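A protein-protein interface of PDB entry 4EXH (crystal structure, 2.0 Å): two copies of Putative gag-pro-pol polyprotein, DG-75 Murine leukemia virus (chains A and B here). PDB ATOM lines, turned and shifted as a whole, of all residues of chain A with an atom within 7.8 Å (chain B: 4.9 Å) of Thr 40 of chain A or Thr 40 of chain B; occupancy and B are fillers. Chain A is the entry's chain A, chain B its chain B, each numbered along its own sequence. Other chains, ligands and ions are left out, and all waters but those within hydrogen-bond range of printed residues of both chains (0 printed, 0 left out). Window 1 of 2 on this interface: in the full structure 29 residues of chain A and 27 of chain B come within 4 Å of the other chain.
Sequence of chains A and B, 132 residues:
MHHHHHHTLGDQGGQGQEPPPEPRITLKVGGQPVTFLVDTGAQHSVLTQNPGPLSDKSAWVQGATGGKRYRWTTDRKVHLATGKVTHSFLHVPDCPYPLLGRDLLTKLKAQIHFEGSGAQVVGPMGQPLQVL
Among the printed residues, pairs that only touch across the chains: Pro 21 of chain A with Arg 102 of chain B (3.5 Å), Pro 23 of chain A with Arg 102 of chain B (3.8 Å), Leu 37 of chain A with Gly 41 of chain B (3.9 Å), Val 38 of chain A with Gly 41 of chain B (3.9 Å), Asp 39 of chain A with Thr 40 of chain B (3.4 Å), Thr 40 of chain A with Pro 23 of chain B (3.9 Å), Thr 40 of chain A with Asp 39 of chain B (3.3 Å), Thr 40 of chain A with Phe 114 of chain B (3.8 Å), Arg 102 of chain A with Pro 23 of chain B (3.98 Å), Leu 105 of chain A with Phe 114 of chain B (3.7 Å), Ala 110 of chain A with Ile 112 of chain B (3.8 Å), Phe 114 of chain A with Thr 40 of chain B (3.7 Å), Phe 114 of chain A with Arg 102 of chain B (3.98 Å) and Phe 114 of chain A with Leu 105 of chain B (3.6 Å).
OE1 of Glu 22 of chain A lies within hydrogen-bond range of N of Ala 119 of chain A (2.8 Å). O of Pro 23 of chain A is in hydrogen-bond range of N of Val 38 of chain A. The backbone carbonyl oxygen of Leu 37 of chain A is in hydrogen-bond range of the backbone NH of Leu 100 of chain A (2.9 Å). NH1 of Arg 102 of chain A sits at hydrogen-bond distance from O of Thr 40 of chain A (3.0 Å). O of Pro 23 of chain B is in hydrogen-bond range of N of Val 38 of chain B, 2.9 Å away. The backbone carbonyl oxygen (O) of Leu 100 of chain B is in hydrogen-bond range of the backbone NH (N) of Asp 39 of chain B, 2.8 Å away.
Hydrophobic or aromatic side chains of chain B within 4 Å of the printed part of chain A: Pro 23, Leu 105 and Phe 114. Of the 21 printed residues of chain A, 13 touch a printed residue of chain B. Among the printed residues, no Asp or Glu carboxylate lies within 4 Å of a Lys or Arg side-chain nitrogen of the other chain.
Of chain B, only Pro 23, Val 38, Asp 39, Thr 40 and Phe 114 come within 4 Å of Thr 40 of chain A. Of the printed residues of chain A, Thr 40 of chain B touches Val 38 (2.6 Å), Asp 39 (3.4 Å), Thr 40 (3.0 Å) and Phe 114 (3.7 Å). Of the printed residues of chain B, Arg 102 of chain A touches Pro 23 (3.98 Å). Printed residues of chain B within 4 Å of Pro 23 of chain A: Arg 102 (3.8 Å). Of the printed residues of chain B, Pro 21 of chain A touches Arg 102. Of the printed residues of chain B, Ile 112 of chain A touches Ile 112. Of the printed residues of chain A, Pro 23 of chain B touches Thr 40 (3.9 Å) and Arg 102 (3.98 Å). Gln 43 of chain A touches none of the printed residues of chain B. Gly 101 of chain A touches none of the printed residues of chain B. The nearest residue of chain B that does not touch Thr 40 of chain A is Leu 37 of chain B (4.3 Å).
Val 38 of chain A touches Thr 40 of chain B, and with the chains exchanged Thr 40 of chain A touches Val 38 of chain B. Thr 40 of chain A touches Pro 23 of chain B, but with the chains exchanged Pro 23 of chain A does not touch Thr 40 of chain B (4.004 Å). Ile 112 of chain A touches its own counterpart, Ile 112 of chain B. Phe 114 of chain A touches Arg 102 of chain B, but with the chains exchanged Arg 102 of chain A does not touch Phe 114 of chain B (4.1 Å). Of the 23 pairs that touch across the chains among the printed residues, 15 have their exchanged pair printed and touching as well.
The backbone carbonyl oxygen of Glu 22 of chain A sits close to the guanidinium group of Arg 102 of chain B, 3.5 Å away. O of Val 38 of chain A lies within hydrogen-bond range of OG1 of Thr 40 of chain B. The side-chain carboxylate (OD1) of Asp 39 of chain B sits close to the side-chain carboxylate (OD1) of Asp 39 of chain A, 2.5 Å away. The side-chain carboxylate (OD1) of Asp 39 of chain A lies close to the backbone NH (N) of Gly 41 of chain B (3.3 Å). The side-chain hydroxyl (OG1) of Thr 40 of chain A lies within hydrogen-bond range of the backbone carbonyl oxygen (O) of Val 38 of chain B (2.7 Å). OG1 of Thr 40 of chain B sits at hydrogen-bond distance from N of Thr 40 of chain A (3.0 Å). OD1 of Asp 39 of chain B lies within hydrogen-bond range of N of Gly 41 of chain A (3.0 Å). O of Ala 110 of chain A lies within hydrogen-bond range of N of Phe 114 of chain B. The backbone NH (N) of Ile 112 of chain A sits at hydrogen-bond distance from the backbone carbonyl oxygen (O) of Ile 112 of chain B (2.9 Å).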
ATOM      1  N   PRO A  21      23.386 -21.610   1.691  1.00  0.00           N
ATOM      2  CA  PRO A  21      23.641 -21.700   3.120  1.00  0.00           C
ATOM      3  C   PRO A  21      22.350 -21.852   3.936  1.00  0.00           C
ATOM      4  O   PRO A  21      21.250 -21.657   3.411  1.00  0.00           O
ATOM      5  CB  PRO A  21      24.297 -20.357   3.440  1.00  0.00           C
ATOM      6  CG  PRO A  21      23.808 -19.434   2.364  1.00  0.00           C
ATOM      7  CD  PRO A  21      23.729 -20.282   1.150  1.00  0.00           C
ATOM      8  N   GLU A  22      22.505 -22.203   5.208  1.00  0.00           N
ATOM      9  CA  GLU A  22      21.409 -22.189   6.167  1.00  0.00           C
ATOM     10  C   GLU A  22      21.004 -20.735   6.392  1.00  0.00           C
ATOM     11  O   GLU A  22      21.859 -19.848   6.289  1.00  0.00           O
ATOM     12  CB  GLU A  22      21.880 -22.794   7.490  1.00  0.00           C
ATOM     13  CG  GLU A  22      22.182 -24.301   7.434  1.00  0.00           C
ATOM     14  CD  GLU A  22      22.324 -24.939   8.826  1.00  0.00           C
ATOM     15  OE1 GLU A  22      22.497 -24.211   9.832  1.00  0.00           O
ATOM     16  OE2 GLU A  22      22.254 -26.182   8.921  1.00  0.00           O
ATOM     17  N   PRO A  23      19.713 -20.471   6.690  1.00  0.00           N
ATOM     18  CA  PRO A  23      18.590 -21.407   6.755  1.00  0.00           C
ATOM     19  C   PRO A  23      18.123 -21.760   5.350  1.00  0.00           C
ATOM     20  O   PRO A  23      18.009 -20.877   4.498  1.00  0.00           O
ATOM     21  CB  PRO A  23      17.506 -20.617   7.491  1.00  0.00           C
ATOM     22  CG  PRO A  23      17.813 -19.188   7.195  1.00  0.00           C
ATOM     23  CD  PRO A  23      19.319 -19.113   7.108  1.00  0.00           C
ATOM     24  N   LEU A  37      17.260 -20.968  -0.390  1.00  0.00           N
ATOM     25  CA  LEU A  37      17.681 -20.129   0.738  1.00  0.00           C
ATOM     26  C   LEU A  37      16.425 -19.454   1.258  1.00  0.00           C
ATOM     27  O   LEU A  37      15.654 -18.878   0.482  1.00  0.00           O
ATOM     28  CB  LEU A  37      18.708 -19.080   0.320  1.00  0.00           C
ATOM     29  CG  LEU A  37      19.044 -17.969   1.326  1.00  0.00           C
ATOM     30  CD1 LEU A  37      19.693 -18.538   2.589  1.00  0.00           C
ATOM     31  CD2 LEU A  37      19.962 -16.940   0.675  1.00  0.00           C
ATOM     32  N   VAL A  38      16.212 -19.554   2.566  1.00  0.00           N
ATOM     33  CA  VAL A  38      15.093 -18.891   3.199  1.00  0.00           C
ATOM     34  C   VAL A  38      15.466 -17.421   3.387  1.00  0.00           C
ATOM     35  O   VAL A  38      16.453 -17.080   4.074  1.00  0.00           O
ATOM     36  CB  VAL A  38      14.688 -19.577   4.516  1.00  0.00           C
ATOM     37  CG1 VAL A  38      13.709 -18.723   5.280  1.00  0.00           C
ATOM     38  CG2 VAL A  38      14.078 -20.940   4.225  1.00  0.00           C
ATOM     39  N   ASP A  39      14.678 -16.554   2.762  1.00  0.00           N
ATOM     40  CA  ASP A  39      15.079 -15.161   2.604  1.00  0.00           C
ATOM     41  C   ASP A  39      13.985 -14.221   3.054  1.00  0.00           C
ATOM     42  O   ASP A  39      13.122 -13.868   2.257  1.00  0.00           O
ATOM     43  CB  ASP A  39      15.409 -14.890   1.134  1.00  0.00           C
ATOM     44  CG  ASP A  39      16.085 -13.543   0.923  1.00  0.00           C
ATOM     45  OD1 ASP A  39      16.255 -12.782   1.902  1.00  0.00           O
ATOM     46  OD2 ASP A  39      16.461 -13.245  -0.236  1.00  0.00           O
ATOM     47  N   THR A  40      14.043 -13.791   4.315  1.00  0.00           N
ATOM     48  CA  THR A  40      13.034 -12.886   4.865  1.00  0.00           C
ATOM     49  C   THR A  40      13.114 -11.499   4.235  1.00  0.00           C
ATOM     50  O   THR A  40      12.173 -10.703   4.335  1.00  0.00           O
ATOM     51  CB  THR A  40      13.126 -12.784   6.390  1.00  0.00           C
ATOM     52  OG1 THR A  40      14.423 -12.288   6.754  1.00  0.00           O
ATOM     53  CG2 THR A  40      12.866 -14.165   7.029  1.00  0.00           C
ATOM     54  N   GLY A  41      14.233 -11.223   3.569  1.00  0.00           N
ATOM     55  CA  GLY A  41      14.406  -9.967   2.837  1.00  0.00           C
ATOM     56  C   GLY A  41      13.803  -9.954   1.433  1.00  0.00           C
ATOM     57  O   GLY A  41      13.770  -8.903   0.778  1.00  0.00           O
ATOM     58  N   ALA A  42      13.336 -11.106   0.958  1.00  0.00           N
ATOM     59  CA  ALA A  42      12.723 -11.178  -0.368  1.00  0.00           C
ATOM     60  C   ALA A  42      11.202 -11.040  -0.289  1.00  0.00           C
ATOM     61  O   ALA A  42      10.535 -11.750   0.458  1.00  0.00           O
ATOM     62  CB  ALA A  42      13.107 -12.460  -1.049  1.00  0.00           C
ATOM     63  N   GLN A  43      10.653 -10.109  -1.055  1.00  0.00           N
ATOM     64  CA  GLN A  43       9.214  -9.900  -1.078  1.00  0.00           C
ATOM     65  C   GLN A  43       8.492 -11.046  -1.819  1.00  0.00           C
ATOM     66  O   GLN A  43       7.409 -11.482  -1.420  1.00  0.00           O
ATOM     67  CB  GLN A  43       8.918  -8.544  -1.718  1.00  0.00           C
ATOM     68  CG  GLN A  43       7.450  -8.187  -1.825  1.00  0.00           C
ATOM     69  CD  GLN A  43       7.237  -6.776  -2.359  1.00  0.00           C
ATOM     70  OE1 GLN A  43       8.175  -5.982  -2.468  1.00  0.00           O
ATOM     71  NE2 GLN A  43       5.995  -6.459  -2.675  1.00  0.00           N
ATOM     72  N   LEU A  99      15.188 -18.465  -3.960  1.00  0.00           N
ATOM     73  CA  LEU A  99      14.867 -17.771  -2.719  1.00  0.00           C
ATOM     74  C   LEU A  99      13.439 -18.038  -2.349  1.00  0.00           C
ATOM     75  O   LEU A  99      12.552 -18.026  -3.203  1.00  0.00           O
ATOM     76  CB  LEU A  99      15.073 -16.250  -2.840  1.00  0.00           C
ATOM     77  CG  LEU A  99      16.413 -15.765  -3.376  1.00  0.00           C
ATOM     78  CD1 LEU A  99      16.375 -14.250  -3.546  1.00  0.00           C
ATOM     79  CD2 LEU A  99      17.576 -16.177  -2.475  1.00  0.00           C
ATOM     80  N   LEU A 100      13.232 -18.305  -1.070  1.00  0.00           N
ATOM     81  CA  LEU A 100      11.898 -18.456  -0.525  1.00  0.00           C
ATOM     82  C   LEU A 100      11.586 -17.207   0.282  1.00  0.00           C
ATOM     83  O   LEU A 100      12.126 -16.997   1.380  1.00  0.00           O
ATOM     84  CB  LEU A 100      11.837 -19.724   0.335  1.00  0.00           C
ATOM     85  CG  LEU A 100      10.439 -20.203   0.690  1.00  0.00           C
ATOM     86  CD1 LEU A 100       9.804 -20.867  -0.536  1.00  0.00           C
ATOM     87  CD2 LEU A 100      10.531 -21.173   1.835  1.00  0.00           C
ATOM     88  N   GLY A 101      10.733 -16.357  -0.281  1.00  0.00           N
ATOM     89  CA  GLY A 101      10.488 -15.048   0.299  1.00  0.00           C
ATOM     90  C   GLY A 101       9.304 -15.023   1.247  1.00  0.00           C
ATOM     91  O   GLY A 101       8.710 -16.070   1.559  1.00  0.00           O
ATOM     92  N   ARG A 102       8.957 -13.808   1.672  1.00  0.00           N
ATOM     93  CA  ARG A 102       7.881 -13.551   2.613  1.00  0.00           C
ATOM     94  C   ARG A 102       6.504 -14.005   2.101  1.00  0.00           C
ATOM     95  O   ARG A 102       5.636 -14.346   2.901  1.00  0.00           O
ATOM     96  CB  ARG A 102       7.838 -12.062   2.987  1.00  0.00           C
ATOM     97  CG  ARG A 102       9.075 -11.573   3.723  1.00  0.00           C
ATOM     98  CD  ARG A 102       8.877 -10.176   4.319  1.00  0.00           C
ATOM     99  NE  ARG A 102       8.509  -9.147   3.348  1.00  0.00           N
ATOM    100  CZ  ARG A 102       9.378  -8.446   2.627  1.00  0.00           C
ATOM    101  NH1 ARG A 102      10.682  -8.645   2.769  1.00  0.00           N
ATOM    102  NH2 ARG A 102       8.943  -7.533   1.768  1.00  0.00           N
ATOM    103  N   ASP A 103       6.315 -14.021   0.783  1.00  0.00           N
ATOM    104  CA  ASP A 103       5.055 -14.495   0.190  1.00  0.00           C
ATOM    105  C   ASP A 103       4.728 -15.967   0.550  1.00  0.00           C
ATOM    106  O   ASP A 103       3.577 -16.297   0.816  1.00  0.00           O
ATOM    107  CB  ASP A 103       5.067 -14.293  -1.335  1.00  0.00           C
ATOM    108  CG  ASP A 103       6.247 -15.015  -2.035  1.00  0.00           C
ATOM    109  OD1 ASP A 103       7.206 -15.460  -1.351  1.00  0.00           O
ATOM    110  OD2 ASP A 103       6.212 -15.141  -3.289  1.00  0.00           O
ATOM    111  N   LEU A 105       6.665 -17.728   3.022  1.00  0.00           N
ATOM    112  CA  LEU A 105       6.919 -17.854   4.451  1.00  0.00           C
ATOM    113  C   LEU A 105       5.663 -17.533   5.243  1.00  0.00           C
ATOM    114  O   LEU A 105       5.390 -18.177   6.255  1.00  0.00           O
ATOM    115  CB  LEU A 105       8.081 -16.967   4.914  1.00  0.00           C
ATOM    116  CG  LEU A 105       9.445 -17.452   4.447  1.00  0.00           C
ATOM    117  CD1 LEU A 105      10.480 -16.346   4.572  1.00  0.00           C
ATOM    118  CD2 LEU A 105       9.836 -18.700   5.246  1.00  0.00           C
ATOM    119  N   ALA A 110       6.271 -20.116   9.020  1.00  0.00           N
ATOM    120  CA  ALA A 110       7.539 -20.667   9.482  1.00  0.00           C
ATOM    121  C   ALA A 110       8.138 -19.885  10.658  1.00  0.00           C
ATOM    122  O   ALA A 110       7.877 -18.689  10.849  1.00  0.00           O
ATOM    123  CB  ALA A 110       8.531 -20.753   8.328  1.00  0.00           C
ATOM    124  N   ILE A 112      12.057 -19.320  12.149  1.00  0.00           N
ATOM    125  CA  ILE A 112      13.458 -19.500  11.806  1.00  0.00           C
ATOM    126  C   ILE A 112      14.297 -19.273  13.066  1.00  0.00           C
ATOM    127  O   ILE A 112      14.170 -18.242  13.719  1.00  0.00           O
ATOM    128  CB  ILE A 112      13.872 -18.543  10.669  1.00  0.00           C
ATOM    129  CG1 ILE A 112      13.009 -18.795   9.423  1.00  0.00           C
ATOM    130  CG2 ILE A 112      15.350 -18.698  10.347  1.00  0.00           C
ATOM    131  CD1 ILE A 112      12.624 -17.529   8.669  1.00  0.00           C
ATOM    132  N   HIS A 113      15.133 -20.246  13.409  1.00  0.00           N
ATOM    133  CA  HIS A 113      15.868 -20.217  14.673  1.00  0.00           C
ATOM    134  C   HIS A 113      17.363 -20.125  14.438  1.00  0.00           C
ATOM    135  O   HIS A 113      17.935 -20.979  13.752  1.00  0.00           O
ATOM    136  CB  HIS A 113      15.568 -21.477  15.494  1.00  0.00           C
ATOM    137  CG  HIS A 113      14.170 -21.538  16.022  1.00  0.00           C
ATOM    138  ND1 HIS A 113      13.884 -21.525  17.369  1.00  0.00           N
ATOM    139  CD2 HIS A 113      12.978 -21.624  15.386  1.00  0.00           C
ATOM    140  CE1 HIS A 113      12.574 -21.593  17.542  1.00  0.00           C
ATOM    141  NE2 HIS A 113      12.002 -21.650  16.353  1.00  0.00           N
ATOM    142  N   PHE A 114      17.986 -19.093  15.007  1.00  0.00           N
ATOM    143  CA  PHE A 114      19.440 -18.920  14.916  1.00  0.00           C
ATOM    144  C   PHE A 114      20.205 -19.342  16.185  1.00  0.00           C
ATOM    145  O   PHE A 114      21.442 -19.310  16.209  1.00  0.00           O
ATOM    146  CB  PHE A 114      19.792 -17.478  14.520  1.00  0.00           C
ATOM    147  CG  PHE A 114      19.601 -17.188  13.061  1.00  0.00           C
ATOM    148  CD1 PHE A 114      20.687 -17.231  12.182  1.00  0.00           C
ATOM    149  CD2 PHE A 114      18.344 -16.863  12.554  1.00  0.00           C
ATOM    150  CE1 PHE A 114      20.524 -16.954  10.816  1.00  0.00           C
ATOM    151  CE2 PHE A 114      18.171 -16.590  11.181  1.00  0.00           C
ATOM    152  CZ  PHE A 114      19.257 -16.638  10.317  1.00  0.00           C
ATOM    153  N   ALA A 119      21.300 -22.388  11.538  1.00  0.00           N
ATOM    154  CA  ALA A 119      19.922 -21.925  11.610  1.00  0.00           C
ATOM    155  C   ALA A 119      18.990 -22.999  11.094  1.00  0.00           C
ATOM    156  O   ALA A 119      19.285 -23.660  10.098  1.00  0.00           O
ATOM    157  CB  ALA A 119      19.741 -20.645  10.813  1.00  0.00           C
ATOM    158  N   PRO B  23       9.858  -8.722   8.633  1.00  0.00           N
ATOM    159  CA  PRO B  23      10.352  -8.541   9.978  1.00  0.00           C
ATOM    160  C   PRO B  23      11.359  -7.398  10.041  1.00  0.00           C
ATOM    161  O   PRO B  23      12.196  -7.256   9.162  1.00  0.00           O
ATOM    162  CB  PRO B  23      11.036  -9.879  10.287  1.00  0.00           C
ATOM    163  CG  PRO B  23      11.407 -10.444   8.983  1.00  0.00           C
ATOM    164  CD  PRO B  23      10.497  -9.853   7.940  1.00  0.00           C
ATOM    165  N   LEU B  37      15.623  -3.910   8.105  1.00  0.00           N
ATOM    166  CA  LEU B  37      14.919  -5.074   7.608  1.00  0.00           C
ATOM    167  C   LEU B  37      15.721  -6.309   8.019  1.00  0.00           C
ATOM    168  O   LEU B  37      16.909  -6.433   7.691  1.00  0.00           O
ATOM    169  CB  LEU B  37      14.783  -5.017   6.079  1.00  0.00           C
ATOM    170  CG  LEU B  37      14.259  -6.252   5.340  1.00  0.00           C
ATOM    171  CD1 LEU B  37      12.897  -6.691   5.831  1.00  0.00           C
ATOM    172  CD2 LEU B  37      14.218  -5.988   3.825  1.00  0.00           C
ATOM    173  N   VAL B  38      15.079  -7.221   8.737  1.00  0.00           N
ATOM    174  CA  VAL B  38      15.736  -8.464   9.114  1.00  0.00           C
ATOM    175  C   VAL B  38      15.751  -9.368   7.884  1.00  0.00           C
ATOM    176  O   VAL B  38      14.695  -9.666   7.299  1.00  0.00           O
ATOM    177  CB  VAL B  38      15.069  -9.110  10.332  1.00  0.00           C
ATOM    178  CG1 VAL B  38      15.674 -10.474  10.616  1.00  0.00           C
ATOM    179  CG2 VAL B  38      15.233  -8.186  11.549  1.00  0.00           C
ATOM    180  N   ASP B  39      16.952  -9.764   7.467  1.00  0.00           N
ATOM    181  CA  ASP B  39      17.122 -10.432   6.182  1.00  0.00           C
ATOM    182  C   ASP B  39      17.993 -11.683   6.304  1.00  0.00           C
ATOM    183  O   ASP B  39      19.226 -11.598   6.324  1.00  0.00           O
ATOM    184  CB  ASP B  39      17.726  -9.462   5.157  1.00  0.00           C
ATOM    185  CG  ASP B  39      17.795 -10.059   3.745  1.00  0.00           C
ATOM    186  OD1 ASP B  39      17.273 -11.182   3.534  1.00  0.00           O
ATOM    187  OD2 ASP B  39      18.355  -9.401   2.840  1.00  0.00           O
ATOM    188  N   THR B  40      17.350 -12.844   6.374  1.00  0.00           N
ATOM    189  CA  THR B  40      18.086 -14.104   6.504  1.00  0.00           C
ATOM    190  C   THR B  40      18.827 -14.414   5.213  1.00  0.00           C
ATOM    191  O   THR B  40      19.695 -15.272   5.193  1.00  0.00           O
ATOM    192  CB  THR B  40      17.158 -15.255   6.825  1.00  0.00           C
ATOM    193  OG1 THR B  40      16.114 -15.276   5.846  1.00  0.00           O
ATOM    194  CG2 THR B  40      16.532 -15.056   8.219  1.00  0.00           C
ATOM    195  N   GLY B  41      18.471 -13.710   4.139  1.00  0.00           N
ATOM    196  CA  GLY B  41      19.154 -13.854   2.850  1.00  0.00           C
ATOM    197  C   GLY B  41      20.412 -13.009   2.724  1.00  0.00           C
ATOM    198  O   GLY B  41      21.102 -13.083   1.711  1.00  0.00           O
ATOM    199  N   ALA B  42      20.715 -12.198   3.742  1.00  0.00           N
ATOM    200  CA  ALA B  42      21.922 -11.375   3.723  1.00  0.00           C
ATOM    201  C   ALA B  42      23.050 -12.050   4.473  1.00  0.00           C
ATOM    202  O   ALA B  42      22.941 -12.297   5.667  1.00  0.00           O
ATOM    203  CB  ALA B  42      21.662  -9.996   4.304  1.00  0.00           C
ATOM    204  N   LEU B 100      19.669  -6.406   8.419  1.00  0.00           N
ATOM    205  CA  LEU B 100      20.270  -7.156   9.490  1.00  0.00           C
ATOM    206  C   LEU B 100      20.390  -8.596   8.998  1.00  0.00           C
ATOM    207  O   LEU B 100      19.380  -9.335   8.886  1.00  0.00           O
ATOM    208  CB  LEU B 100      19.383  -7.057  10.732  1.00  0.00           C
ATOM    209  CG  LEU B 100      19.930  -7.325  12.132  1.00  0.00           C
ATOM    210  CD1 LEU B 100      20.188  -8.776  12.372  1.00  0.00           C
ATOM    211  CD2 LEU B 100      21.177  -6.484  12.377  1.00  0.00           C
ATOM    212  N   ARG B 102      22.672 -12.489   8.442  1.00  0.00           N
ATOM    213  CA  ARG B 102      22.927 -13.698   9.216  1.00  0.00           C
ATOM    214  C   ARG B 102      24.056 -13.545  10.236  1.00  0.00           C
ATOM    215  O   ARG B 102      24.056 -14.248  11.251  1.00  0.00           O
ATOM    216  CB  ARG B 102      23.195 -14.890   8.296  1.00  0.00           C
ATOM    217  CG  ARG B 102      21.970 -15.311   7.487  1.00  0.00           C
ATOM    218  CD  ARG B 102      22.187 -16.659   6.816  1.00  0.00           C
ATOM    219  NE  ARG B 102      23.377 -16.723   5.957  1.00  0.00           N
ATOM    220  CZ  ARG B 102      23.435 -16.301   4.697  1.00  0.00           C
ATOM    221  NH1 ARG B 102      22.381 -15.746   4.099  1.00  0.00           N
ATOM    222  NH2 ARG B 102      24.567 -16.417   4.026  1.00  0.00           N
ATOM    223  N   LEU B 105      22.222 -11.836  13.279  1.00  0.00           N
ATOM    224  CA  LEU B 105      21.203 -12.793  13.677  1.00  0.00           C
ATOM    225  C   LEU B 105      21.817 -13.932  14.507  1.00  0.00           C
ATOM    226  O   LEU B 105      21.247 -14.342  15.522  1.00  0.00           O
ATOM    227  CB  LEU B 105      20.464 -13.327  12.450  1.00  0.00           C
ATOM    228  CG  LEU B 105      19.494 -12.310  11.841  1.00  0.00           C
ATOM    229  CD1 LEU B 105      18.986 -12.789  10.480  1.00  0.00           C
ATOM    230  CD2 LEU B 105      18.343 -11.988  12.798  1.00  0.00           C
ATOM    231  N   ILE B 112      12.805 -15.769  14.176  1.00  0.00           N
ATOM    232  CA  ILE B 112      11.851 -15.007  13.380  1.00  0.00           C
ATOM    233  C   ILE B 112      10.562 -15.815  13.240  1.00  0.00           C
ATOM    234  O   ILE B 112      10.590 -16.967  12.814  1.00  0.00           O
ATOM    235  CB  ILE B 112      12.436 -14.646  11.990  1.00  0.00           C
ATOM    236  CG1 ILE B 112      13.694 -13.788  12.155  1.00  0.00           C
ATOM    237  CG2 ILE B 112      11.414 -13.899  11.148  1.00  0.00           C
ATOM    238  CD1 ILE B 112      14.701 -13.990  11.054  1.00  0.00           C
ATOM    239  N   PHE B 114       6.708 -16.039  11.616  1.00  0.00           N
ATOM    240  CA  PHE B 114       5.660 -15.561  10.715  1.00  0.00           C
ATOM    241  C   PHE B 114       4.288 -15.951  11.268  1.00  0.00           C
ATOM    242  O   PHE B 114       4.031 -17.118  11.539  1.00  0.00           O
ATOM    243  CB  PHE B 114       5.873 -16.085   9.292  1.00  0.00           C
ATOM    244  CG  PHE B 114       6.967 -15.372   8.552  1.00  0.00           C
ATOM    245  CD1 PHE B 114       6.659 -14.381   7.621  1.00  0.00           C
ATOM    246  CD2 PHE B 114       8.307 -15.673   8.801  1.00  0.00           C
ATOM    247  CE1 PHE B 114       7.670 -13.702   6.939  1.00  0.00           C
ATOM    248  CE2 PHE B 114       9.327 -15.003   8.130  1.00  0.00           C
ATOM    249  CZ  PHE B 114       9.009 -14.012   7.197  1.00  0.00           C
